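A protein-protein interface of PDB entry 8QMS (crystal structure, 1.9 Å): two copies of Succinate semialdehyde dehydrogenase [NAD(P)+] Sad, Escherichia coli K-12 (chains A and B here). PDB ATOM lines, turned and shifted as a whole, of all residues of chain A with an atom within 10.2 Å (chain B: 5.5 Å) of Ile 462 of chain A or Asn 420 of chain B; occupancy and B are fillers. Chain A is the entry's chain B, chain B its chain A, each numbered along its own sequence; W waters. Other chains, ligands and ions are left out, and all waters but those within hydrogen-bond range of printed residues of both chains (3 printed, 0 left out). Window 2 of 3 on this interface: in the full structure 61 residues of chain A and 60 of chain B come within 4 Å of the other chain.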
ATOM      1  N   VAL A 115     -29.440  41.771 -22.717  1.00  0.00           N
ATOM      2  CA  VAL A 115     -30.308  40.602 -22.768  1.00  0.00           C
ATOM      3  C   VAL A 115     -31.178  40.552 -21.516  1.00  0.00           C
ATOM      4  O   VAL A 115     -30.720  40.840 -20.402  1.00  0.00           O
ATOM      5  CB  VAL A 115     -29.476  39.317 -22.926  1.00  0.00           C
ATOM      6  CG1 VAL A 115     -30.360  38.073 -22.776  1.00  0.00           C
ATOM      7  CG2 VAL A 115     -28.777  39.298 -24.277  1.00  0.00           C
ATOM      8  N   GLU A 116     -32.444  40.176 -21.706  1.00  0.00           N
ATOM      9  CA  GLU A 116     -33.404  40.078 -20.612  1.00  0.00           C
ATOM     10  C   GLU A 116     -32.902  39.174 -19.490  1.00  0.00           C
ATOM     11  O   GLU A 116     -32.155  38.215 -19.713  1.00  0.00           O
ATOM     12  CB  GLU A 116     -34.743  39.548 -21.139  1.00  0.00           C
ATOM     13  CG  GLU A 116     -34.631  38.255 -21.944  1.00  0.00           C
ATOM     14  CD  GLU A 116     -34.381  38.497 -23.428  1.00  0.00           C
ATOM     15  OE1 GLU A 116     -34.441  39.668 -23.859  1.00  0.00           O
ATOM     16  OE2 GLU A 116     -34.133  37.510 -24.165  1.00  0.00           O
ATOM     17  N   ASN A 117     -33.332  39.495 -18.266  1.00  0.00           N
ATOM     18  CA  ASN A 117     -33.120  38.672 -17.075  1.00  0.00           C
ATOM     19  C   ASN A 117     -31.647  38.519 -16.714  1.00  0.00           C
ATOM     20  O   ASN A 117     -31.288  37.594 -15.975  1.00  0.00           O
ATOM     21  CB  ASN A 117     -33.759  37.287 -17.233  1.00  0.00           C
ATOM     22  CG  ASN A 117     -35.233  37.360 -17.561  1.00  0.00           C
ATOM     23  OD1 ASN A 117     -35.723  36.643 -18.435  1.00  0.00           O
ATOM     24  ND2 ASN A 117     -35.950  38.230 -16.862  1.00  0.00           N
ATOM     25  N   GLN A 119     -29.336  37.357 -18.375  1.00  0.00           N
ATOM     26  CA  GLN A 119     -28.989  35.987 -18.740  1.00  0.00           C
ATOM     27  C   GLN A 119     -27.610  35.882 -19.369  1.00  0.00           C
ATOM     28  O   GLN A 119     -26.982  34.818 -19.293  1.00  0.00           O
ATOM     29  CB  GLN A 119     -30.016  35.425 -19.721  1.00  0.00           C
ATOM     30  CG  GLN A 119     -31.356  35.081 -19.129  1.00  0.00           C
ATOM     31  CD  GLN A 119     -32.334  34.607 -20.189  1.00  0.00           C
ATOM     32  OE1 GLN A 119     -32.071  34.719 -21.397  1.00  0.00           O
ATOM     33  NE2 GLN A 119     -33.470  34.082 -19.749  1.00  0.00           N
ATOM     34  N   VAL A 457     -21.304  34.265 -22.354  1.00  0.00           N
ATOM     35  CA  VAL A 457     -21.876  33.184 -21.556  1.00  0.00           C
ATOM     36  C   VAL A 457     -23.343  33.517 -21.338  1.00  0.00           C
ATOM     37  O   VAL A 457     -23.667  34.512 -20.677  1.00  0.00           O
ATOM     38  CB  VAL A 457     -21.153  32.991 -20.214  1.00  0.00           C
ATOM     39  CG1 VAL A 457     -21.733  31.793 -19.476  1.00  0.00           C
ATOM     40  CG2 VAL A 457     -19.645  32.820 -20.423  1.00  0.00           C
ATOM     41  N   TRP A 458     -24.227  32.693 -21.898  1.00  0.00           N
ATOM     42  CA  TRP A 458     -25.652  32.996 -21.973  1.00  0.00           C
ATOM     43  C   TRP A 458     -26.410  31.832 -21.353  1.00  0.00           C
ATOM     44  O   TRP A 458     -26.391  30.721 -21.892  1.00  0.00           O
ATOM     45  CB  TRP A 458     -26.076  33.232 -23.426  1.00  0.00           C
ATOM     46  CG  TRP A 458     -27.433  33.860 -23.620  1.00  0.00           C
ATOM     47  CD1 TRP A 458     -28.494  33.834 -22.755  1.00  0.00           C
ATOM     48  CD2 TRP A 458     -27.867  34.610 -24.764  1.00  0.00           C
ATOM     49  NE1 TRP A 458     -29.559  34.522 -23.294  1.00  0.00           N
ATOM     50  CE2 TRP A 458     -29.198  35.009 -24.525  1.00  0.00           C
ATOM     51  CE3 TRP A 458     -27.253  34.989 -25.963  1.00  0.00           C
ATOM     52  CZ2 TRP A 458     -29.928  35.763 -25.445  1.00  0.00           C
ATOM     53  CZ3 TRP A 458     -27.979  35.738 -26.875  1.00  0.00           C
ATOM     54  CH2 TRP A 458     -29.304  36.114 -26.611  1.00  0.00           C
ATOM     55  N   LYS A 459     -27.066  32.089 -20.223  1.00  0.00           N
ATOM     56  CA  LYS A 459     -27.809  31.076 -19.484  1.00  0.00           C
ATOM     57  C   LYS A 459     -29.298  31.154 -19.815  1.00  0.00           C
ATOM     58  O   LYS A 459     -29.859  32.245 -19.937  1.00  0.00           O
ATOM     59  CB  LYS A 459     -27.596  31.258 -17.978  1.00  0.00           C
ATOM     60  CG  LYS A 459     -28.375  30.294 -17.103  1.00  0.00           C
ATOM     61  CD  LYS A 459     -28.066  30.481 -15.614  1.00  0.00           C
ATOM     62  CE  LYS A 459     -28.499  31.853 -15.101  1.00  0.00           C
ATOM     63  NZ  LYS A 459     -28.296  31.978 -13.623  1.00  0.00           N
ATOM     64  N   ASP A 460     -29.932  29.984 -19.963  1.00  0.00           N
ATOM     65  CA  ASP A 460     -31.391  29.874 -20.084  1.00  0.00           C
ATOM     66  C   ASP A 460     -31.943  30.646 -21.281  1.00  0.00           C
ATOM     67  O   ASP A 460     -32.988  31.295 -21.187  1.00  0.00           O
ATOM     68  CB  ASP A 460     -32.094  30.335 -18.805  1.00  0.00           C
ATOM     69  CG  ASP A 460     -31.644  29.572 -17.577  1.00  0.00           C
ATOM     70  OD1 ASP A 460     -31.406  28.350 -17.676  1.00  0.00           O
ATOM     71  OD2 ASP A 460     -31.517  30.207 -16.508  1.00  0.00           O
ATOM     72  N   ARG A 461     -31.262  30.573 -22.423  1.00  0.00           N
ATOM     73  CA  ARG A 461     -31.819  31.186 -23.628  1.00  0.00           C
ATOM     74  C   ARG A 461     -32.847  30.216 -24.200  1.00  0.00           C
ATOM     75  O   ARG A 461     -32.548  29.398 -25.072  1.00  0.00           O
ATOM     76  CB  ARG A 461     -30.740  31.525 -24.652  1.00  0.00           C
ATOM     77  CG  ARG A 461     -31.292  32.392 -25.781  1.00  0.00           C
ATOM     78  CD  ARG A 461     -30.346  32.576 -26.959  1.00  0.00           C
ATOM     79  NE  ARG A 461     -31.025  33.275 -28.048  1.00  0.00           N
ATOM     80  CZ  ARG A 461     -31.727  32.677 -29.001  1.00  0.00           C
ATOM     81  NH1 ARG A 461     -31.824  31.357 -29.064  1.00  0.00           N
ATOM     82  NH2 ARG A 461     -32.354  33.418 -29.909  1.00  0.00           N
ATOM     83  N   ILE A 462     -34.074  30.304 -23.693  1.00  0.00           N
ATOM     84  CA  ILE A 462     -35.144  29.393 -24.104  1.00  0.00           C
ATOM     85  C   ILE A 462     -36.422  30.162 -24.415  1.00  0.00           C
ATOM     86  O   ILE A 462     -36.487  31.386 -24.293  1.00  0.00           O
ATOM     87  CB  ILE A 462     -35.425  28.320 -23.028  1.00  0.00           C
ATOM     88  CG1 ILE A 462     -35.898  28.971 -21.728  1.00  0.00           C
ATOM     89  CG2 ILE A 462     -34.199  27.442 -22.785  1.00  0.00           C
ATOM     90  CD1 ILE A 462     -36.362  27.972 -20.685  1.00  0.00           C
ATOM     91  OXT ILE A 462     -37.432  29.566 -24.796  1.00  0.00           O
ATOM     92  N   LEU B 251     -35.694  19.148 -22.537  1.00  0.00           N
ATOM     93  CA  LEU B 251     -35.214  20.416 -23.075  1.00  0.00           C
ATOM     94  C   LEU B 251     -33.905  20.231 -23.830  1.00  0.00           C
ATOM     95  O   LEU B 251     -33.684  20.865 -24.871  1.00  0.00           O
ATOM     96  CB  LEU B 251     -35.039  21.434 -21.948  1.00  0.00           C
ATOM     97  CG  LEU B 251     -34.605  22.847 -22.345  1.00  0.00           C
ATOM     98  CD1 LEU B 251     -35.660  23.502 -23.230  1.00  0.00           C
ATOM     99  CD2 LEU B 251     -34.332  23.686 -21.109  1.00  0.00           C
ATOM    100  N   THR B 396     -22.493  24.382 -26.038  1.00  0.00           N
ATOM    101  CA  THR B 396     -23.661  24.255 -25.175  1.00  0.00           C
ATOM    102  C   THR B 396     -23.377  23.243 -24.070  1.00  0.00           C
ATOM    103  O   THR B 396     -22.770  22.197 -24.316  1.00  0.00           O
ATOM    104  CB  THR B 396     -24.908  23.812 -25.970  1.00  0.00           C
ATOM    105  OG1 THR B 396     -25.096  24.675 -27.097  1.00  0.00           O
ATOM    106  CG2 THR B 396     -26.158  23.865 -25.094  1.00  0.00           C
ATOM    107  N   ILE B 397     -23.813  23.561 -22.852  1.00  0.00           N
ATOM    108  CA  ILE B 397     -23.765  22.634 -21.724  1.00  0.00           C
ATOM    109  C   ILE B 397     -25.163  22.515 -21.145  1.00  0.00           C
ATOM    110  O   ILE B 397     -25.780  23.526 -20.791  1.00  0.00           O
ATOM    111  CB  ILE B 397     -22.791  23.090 -20.619  1.00  0.00           C
ATOM    112  CG1 ILE B 397     -21.453  23.519 -21.207  1.00  0.00           C
ATOM    113  CG2 ILE B 397     -22.597  21.973 -19.580  1.00  0.00           C
ATOM    114  CD1 ILE B 397     -20.616  24.327 -20.227  1.00  0.00           C
ATOM    115  N   PHE B 398     -25.653  21.284 -21.032  1.00  0.00           N
ATOM    116  CA  PHE B 398     -26.908  21.004 -20.350  1.00  0.00           C
ATOM    117  C   PHE B 398     -26.606  20.250 -19.065  1.00  0.00           C
ATOM    118  O   PHE B 398     -26.066  19.138 -19.104  1.00  0.00           O
ATOM    119  CB  PHE B 398     -27.867  20.219 -21.248  1.00  0.00           C
ATOM    120  CG  PHE B 398     -28.840  21.095 -21.975  1.00  0.00           C
ATOM    121  CD1 PHE B 398     -28.500  21.674 -23.189  1.00  0.00           C
ATOM    122  CD2 PHE B 398     -30.077  21.378 -21.427  1.00  0.00           C
ATOM    123  CE1 PHE B 398     -29.387  22.502 -23.852  1.00  0.00           C
ATOM    124  CE2 PHE B 398     -30.970  22.205 -22.090  1.00  0.00           C
ATOM    125  CZ  PHE B 398     -30.622  22.767 -23.298  1.00  0.00           C
ATOM    126  N   THR B 399     -26.939  20.870 -17.936  1.00  0.00           N
ATOM    127  CA  THR B 399     -26.807  20.296 -16.604  1.00  0.00           C
ATOM    128  C   THR B 399     -27.568  21.191 -15.640  1.00  0.00           C
ATOM    129  O   THR B 399     -27.627  22.410 -15.830  1.00  0.00           O
ATOM    130  CB  THR B 399     -25.337  20.167 -16.179  1.00  0.00           C
ATOM    131  OG1 THR B 399     -25.263  19.671 -14.838  1.00  0.00           O
ATOM    132  CG2 THR B 399     -24.628  21.516 -16.252  1.00  0.00           C
ATOM    133  N   THR B 400     -28.175  20.581 -14.621  1.00  0.00           N
ATOM    134  CA  THR B 400     -28.832  21.383 -13.597  1.00  0.00           C
ATOM    135  C   THR B 400     -27.860  21.913 -12.550  1.00  0.00           C
ATOM    136  O   THR B 400     -28.259  22.746 -11.729  1.00  0.00           O
ATOM    137  CB  THR B 400     -29.945  20.587 -12.908  1.00  0.00           C
ATOM    138  OG1 THR B 400     -29.461  19.288 -12.551  1.00  0.00           O
ATOM    139  CG2 THR B 400     -31.149  20.457 -13.832  1.00  0.00           C
ATOM    140  N   PHE B 418     -23.451  28.462 -24.189  1.00  0.00           N
ATOM    141  CA  PHE B 418     -24.859  28.521 -23.841  1.00  0.00           C
ATOM    142  C   PHE B 418     -25.133  27.441 -22.806  1.00  0.00           C
ATOM    143  O   PHE B 418     -24.835  26.264 -23.035  1.00  0.00           O
ATOM    144  CB  PHE B 418     -25.739  28.356 -25.080  1.00  0.00           C
ATOM    145  CG  PHE B 418     -25.716  29.558 -25.986  1.00  0.00           C
ATOM    146  CD1 PHE B 418     -24.665  29.755 -26.865  1.00  0.00           C
ATOM    147  CD2 PHE B 418     -26.724  30.508 -25.928  1.00  0.00           C
ATOM    148  CE1 PHE B 418     -24.626  30.877 -27.685  1.00  0.00           C
ATOM    149  CE2 PHE B 418     -26.691  31.630 -26.746  1.00  0.00           C
ATOM    150  CZ  PHE B 418     -25.640  31.812 -27.624  1.00  0.00           C
ATOM    151  N   ILE B 419     -25.664  27.852 -21.662  1.00  0.00           N
ATOM    152  CA  ILE B 419     -25.984  26.947 -20.570  1.00  0.00           C
ATOM    153  C   ILE B 419     -27.489  26.726 -20.576  1.00  0.00           C
ATOM    154  O   ILE B 419     -28.266  27.682 -20.459  1.00  0.00           O
ATOM    155  CB  ILE B 419     -25.505  27.504 -19.222  1.00  0.00           C
ATOM    156  CG1 ILE B 419     -23.988  27.721 -19.255  1.00  0.00           C
ATOM    157  CG2 ILE B 419     -25.896  26.557 -18.085  1.00  0.00           C
ATOM    158  CD1 ILE B 419     -23.452  28.558 -18.101  1.00  0.00           C
ATOM    159  N   ASN B 420     -27.897  25.469 -20.736  1.00  0.00           N
ATOM    160  CA  ASN B 420     -29.308  25.079 -20.687  1.00  0.00           C
ATOM    161  C   ASN B 420     -30.164  25.928 -21.630  1.00  0.00           C
ATOM    162  O   ASN B 420     -31.227  26.431 -21.259  1.00  0.00           O
ATOM    163  CB  ASN B 420     -29.835  25.156 -19.252  1.00  0.00           C
ATOM    164  CG  ASN B 420     -29.126  24.194 -18.316  1.00  0.00           C
ATOM    165  OD1 ASN B 420     -28.775  23.077 -18.701  1.00  0.00           O
ATOM    166  ND2 ASN B 420     -28.915  24.623 -17.074  1.00  0.00           N
ATOM    167  N   GLY B 421     -29.701  26.088 -22.866  1.00  0.00           N
ATOM    168  CA  GLY B 421     -30.437  26.919 -23.792  1.00  0.00           C
ATOM    169  C   GLY B 421     -30.062  26.670 -25.236  1.00  0.00           C
ATOM    170  O   GLY B 421     -29.258  25.787 -25.549  1.00  0.00           O
ATOM    171  N   TYR B 422     -30.656  27.483 -26.114  1.00  0.00           N
ATOM    172  CA  TYR B 422     -30.501  27.376 -27.562  1.00  0.00           C
ATOM    173  C   TYR B 422     -29.455  28.376 -28.045  1.00  0.00           C
ATOM    174  O   TYR B 422     -29.662  29.589 -27.948  1.00  0.00           O
ATOM    175  CB  TYR B 422     -31.819  27.656 -28.283  1.00  0.00           C
ATOM    176  CG  TYR B 422     -32.962  26.699 -28.027  1.00  0.00           C
ATOM    177  CD1 TYR B 422     -33.634  26.688 -26.810  1.00  0.00           C
ATOM    178  CD2 TYR B 422     -33.415  25.851 -29.032  1.00  0.00           C
ATOM    179  CE1 TYR B 422     -34.705  25.822 -26.591  1.00  0.00           C
ATOM    180  CE2 TYR B 422     -34.484  24.988 -28.827  1.00  0.00           C
ATOM    181  CZ  TYR B 422     -35.124  24.975 -27.604  1.00  0.00           C
ATOM    182  OH  TYR B 422     -36.185  24.114 -27.397  1.00  0.00           O
HETATM  183  O   HOH W   1     -32.908  26.883 -19.182  1.00  0.00           O
HETATM  184  O   HOH W   2     -28.635  29.435 -22.960  1.00  0.00           O
HETATM  185  O   HOH W   3     -29.619  27.029 -16.126  1.00  0.00           O
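Water W1 lies within hydrogen-bond range of the side-chain carboxylate (OD1) of Asp 460 of chain A (2.6 Å) and the backbone carbonyl oxygen (O) of Asn 420 of chain B (2.7 Å).
Water W3 bridges the side-chain amide nitrogen of Asn 420 of chain B (2.7 Å) and the side-chain carboxylate of Asp 460 of chain A (2.7 Å).
Water W2 lies within hydrogen-bond range of O of Trp 458 of chain A (2.8 Å), N of Arg 461 of chain A (2.9 Å), O of Ile 419 of chain B (3.1 Å) and N of Asp 460 of chain A (3.3 Å).
No position is printed for both chains.
Of the 11 pairs that touch across the chains among the printed residues, none has its exchanged pair printed and touching as well.
NE2 of Gln 119 of chain A is in hydrogen-bond range of O of Asp 460 of chain A (3.2 Å).
The backbone NH (N) of Asn 420 of chain B sits at hydrogen-bond distance from the backbone carbonyl oxygen (O) of Ile 397 of chain B.
NE1 of Trp 458 of chain A lies within hydrogen-bond range of OE1 of Gln 119 of chain A (3.2 Å).
The backbone carbonyl oxygen of Thr 399 of chain B is in hydrogen-bond range of the side-chain amide nitrogen of Asn 420 of chain B (2.8 Å).
O of Gln 119 of chain A sits at hydrogen-bond distance from N of Lys 459 of chain A (2.9 Å).
The backbone NH of Ile 397 of chain B is in hydrogen-bond range of the backbone carbonyl oxygen of Phe 418 of chain B (2.9 Å).
Val 457 of chain A touches Ile 419 of chain B.
Trp 458 of chain A touches Phe 418 of chain B (O to CA, 3.3 Å).
O of Ile 419 of chain B touches CA of Lys 459 of chain A, at 3.6 Å.
CA of Asp 460 of chain A touches O of Asn 420 of chain B, 3.6 Å away.
Arg 461 of chain A touches Phe 418 of chain B (CD to CE2, 3.8 Å).
Gly 421 of chain B touches Arg 461 of chain A.
Ile 462 of chain A touches Asn 420 of chain B.
Ile 462 of chain A touches Gly 421 of chain B (CG2 to CA, 3.9 Å).
Ile 462 of chain A touches two residues of chain B.
Of chain A, only Asp 460 (3.6 Å) and Ile 462 (3.5 Å) come within 4 Å of Asn 420 of chain B.
Gly 421 of chain B touches just these residues of chain A: Arg 461 and Ile 462.
Of the printed residues of chain B, Arg 461 of chain A touches Phe 418, Gly 421 and Tyr 422.
Of the printed residues of chain B, Asp 460 of chain A touches Ile 419 (2.9 Å) and Asn 420 (3.6 Å).
Printed residues of chain B within 4 Å of Trp 458 of chain A: Phe 418 and Ile 419.
Of the printed residues of chain B, Lys 459 of chain A touches Ile 419.
Printed residues of chain A within 4 Å of Tyr 422 of chain B: Arg 461 (2.9 Å).
Ile 397 of chain B touches none of the printed residues of chain A.
Printed residues of chain B that touch a printed residue of chain A: Phe 418, Ile 419, Asn 420, Gly 421 and Tyr 422.
Hydrophobic or aromatic side chains of chain B that line the printed part of chain A: Phe 418, Ile 419 and Tyr 422.
The backbone carbonyl oxygen (O) of Ile 419 of chain B lies within hydrogen-bond range of the backbone NH (N) of Asp 460 of chain A, at 2.9 Å.
The backbone NH of Ile 419 of chain B is in hydrogen-bond range of the backbone carbonyl oxygen of Trp 458 of chain A.
The backbone carbonyl oxygen of Arg 461 of chain A lies within hydrogen-bond range of the backbone NH of Tyr 422 of chain B, at 2.9 Å.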
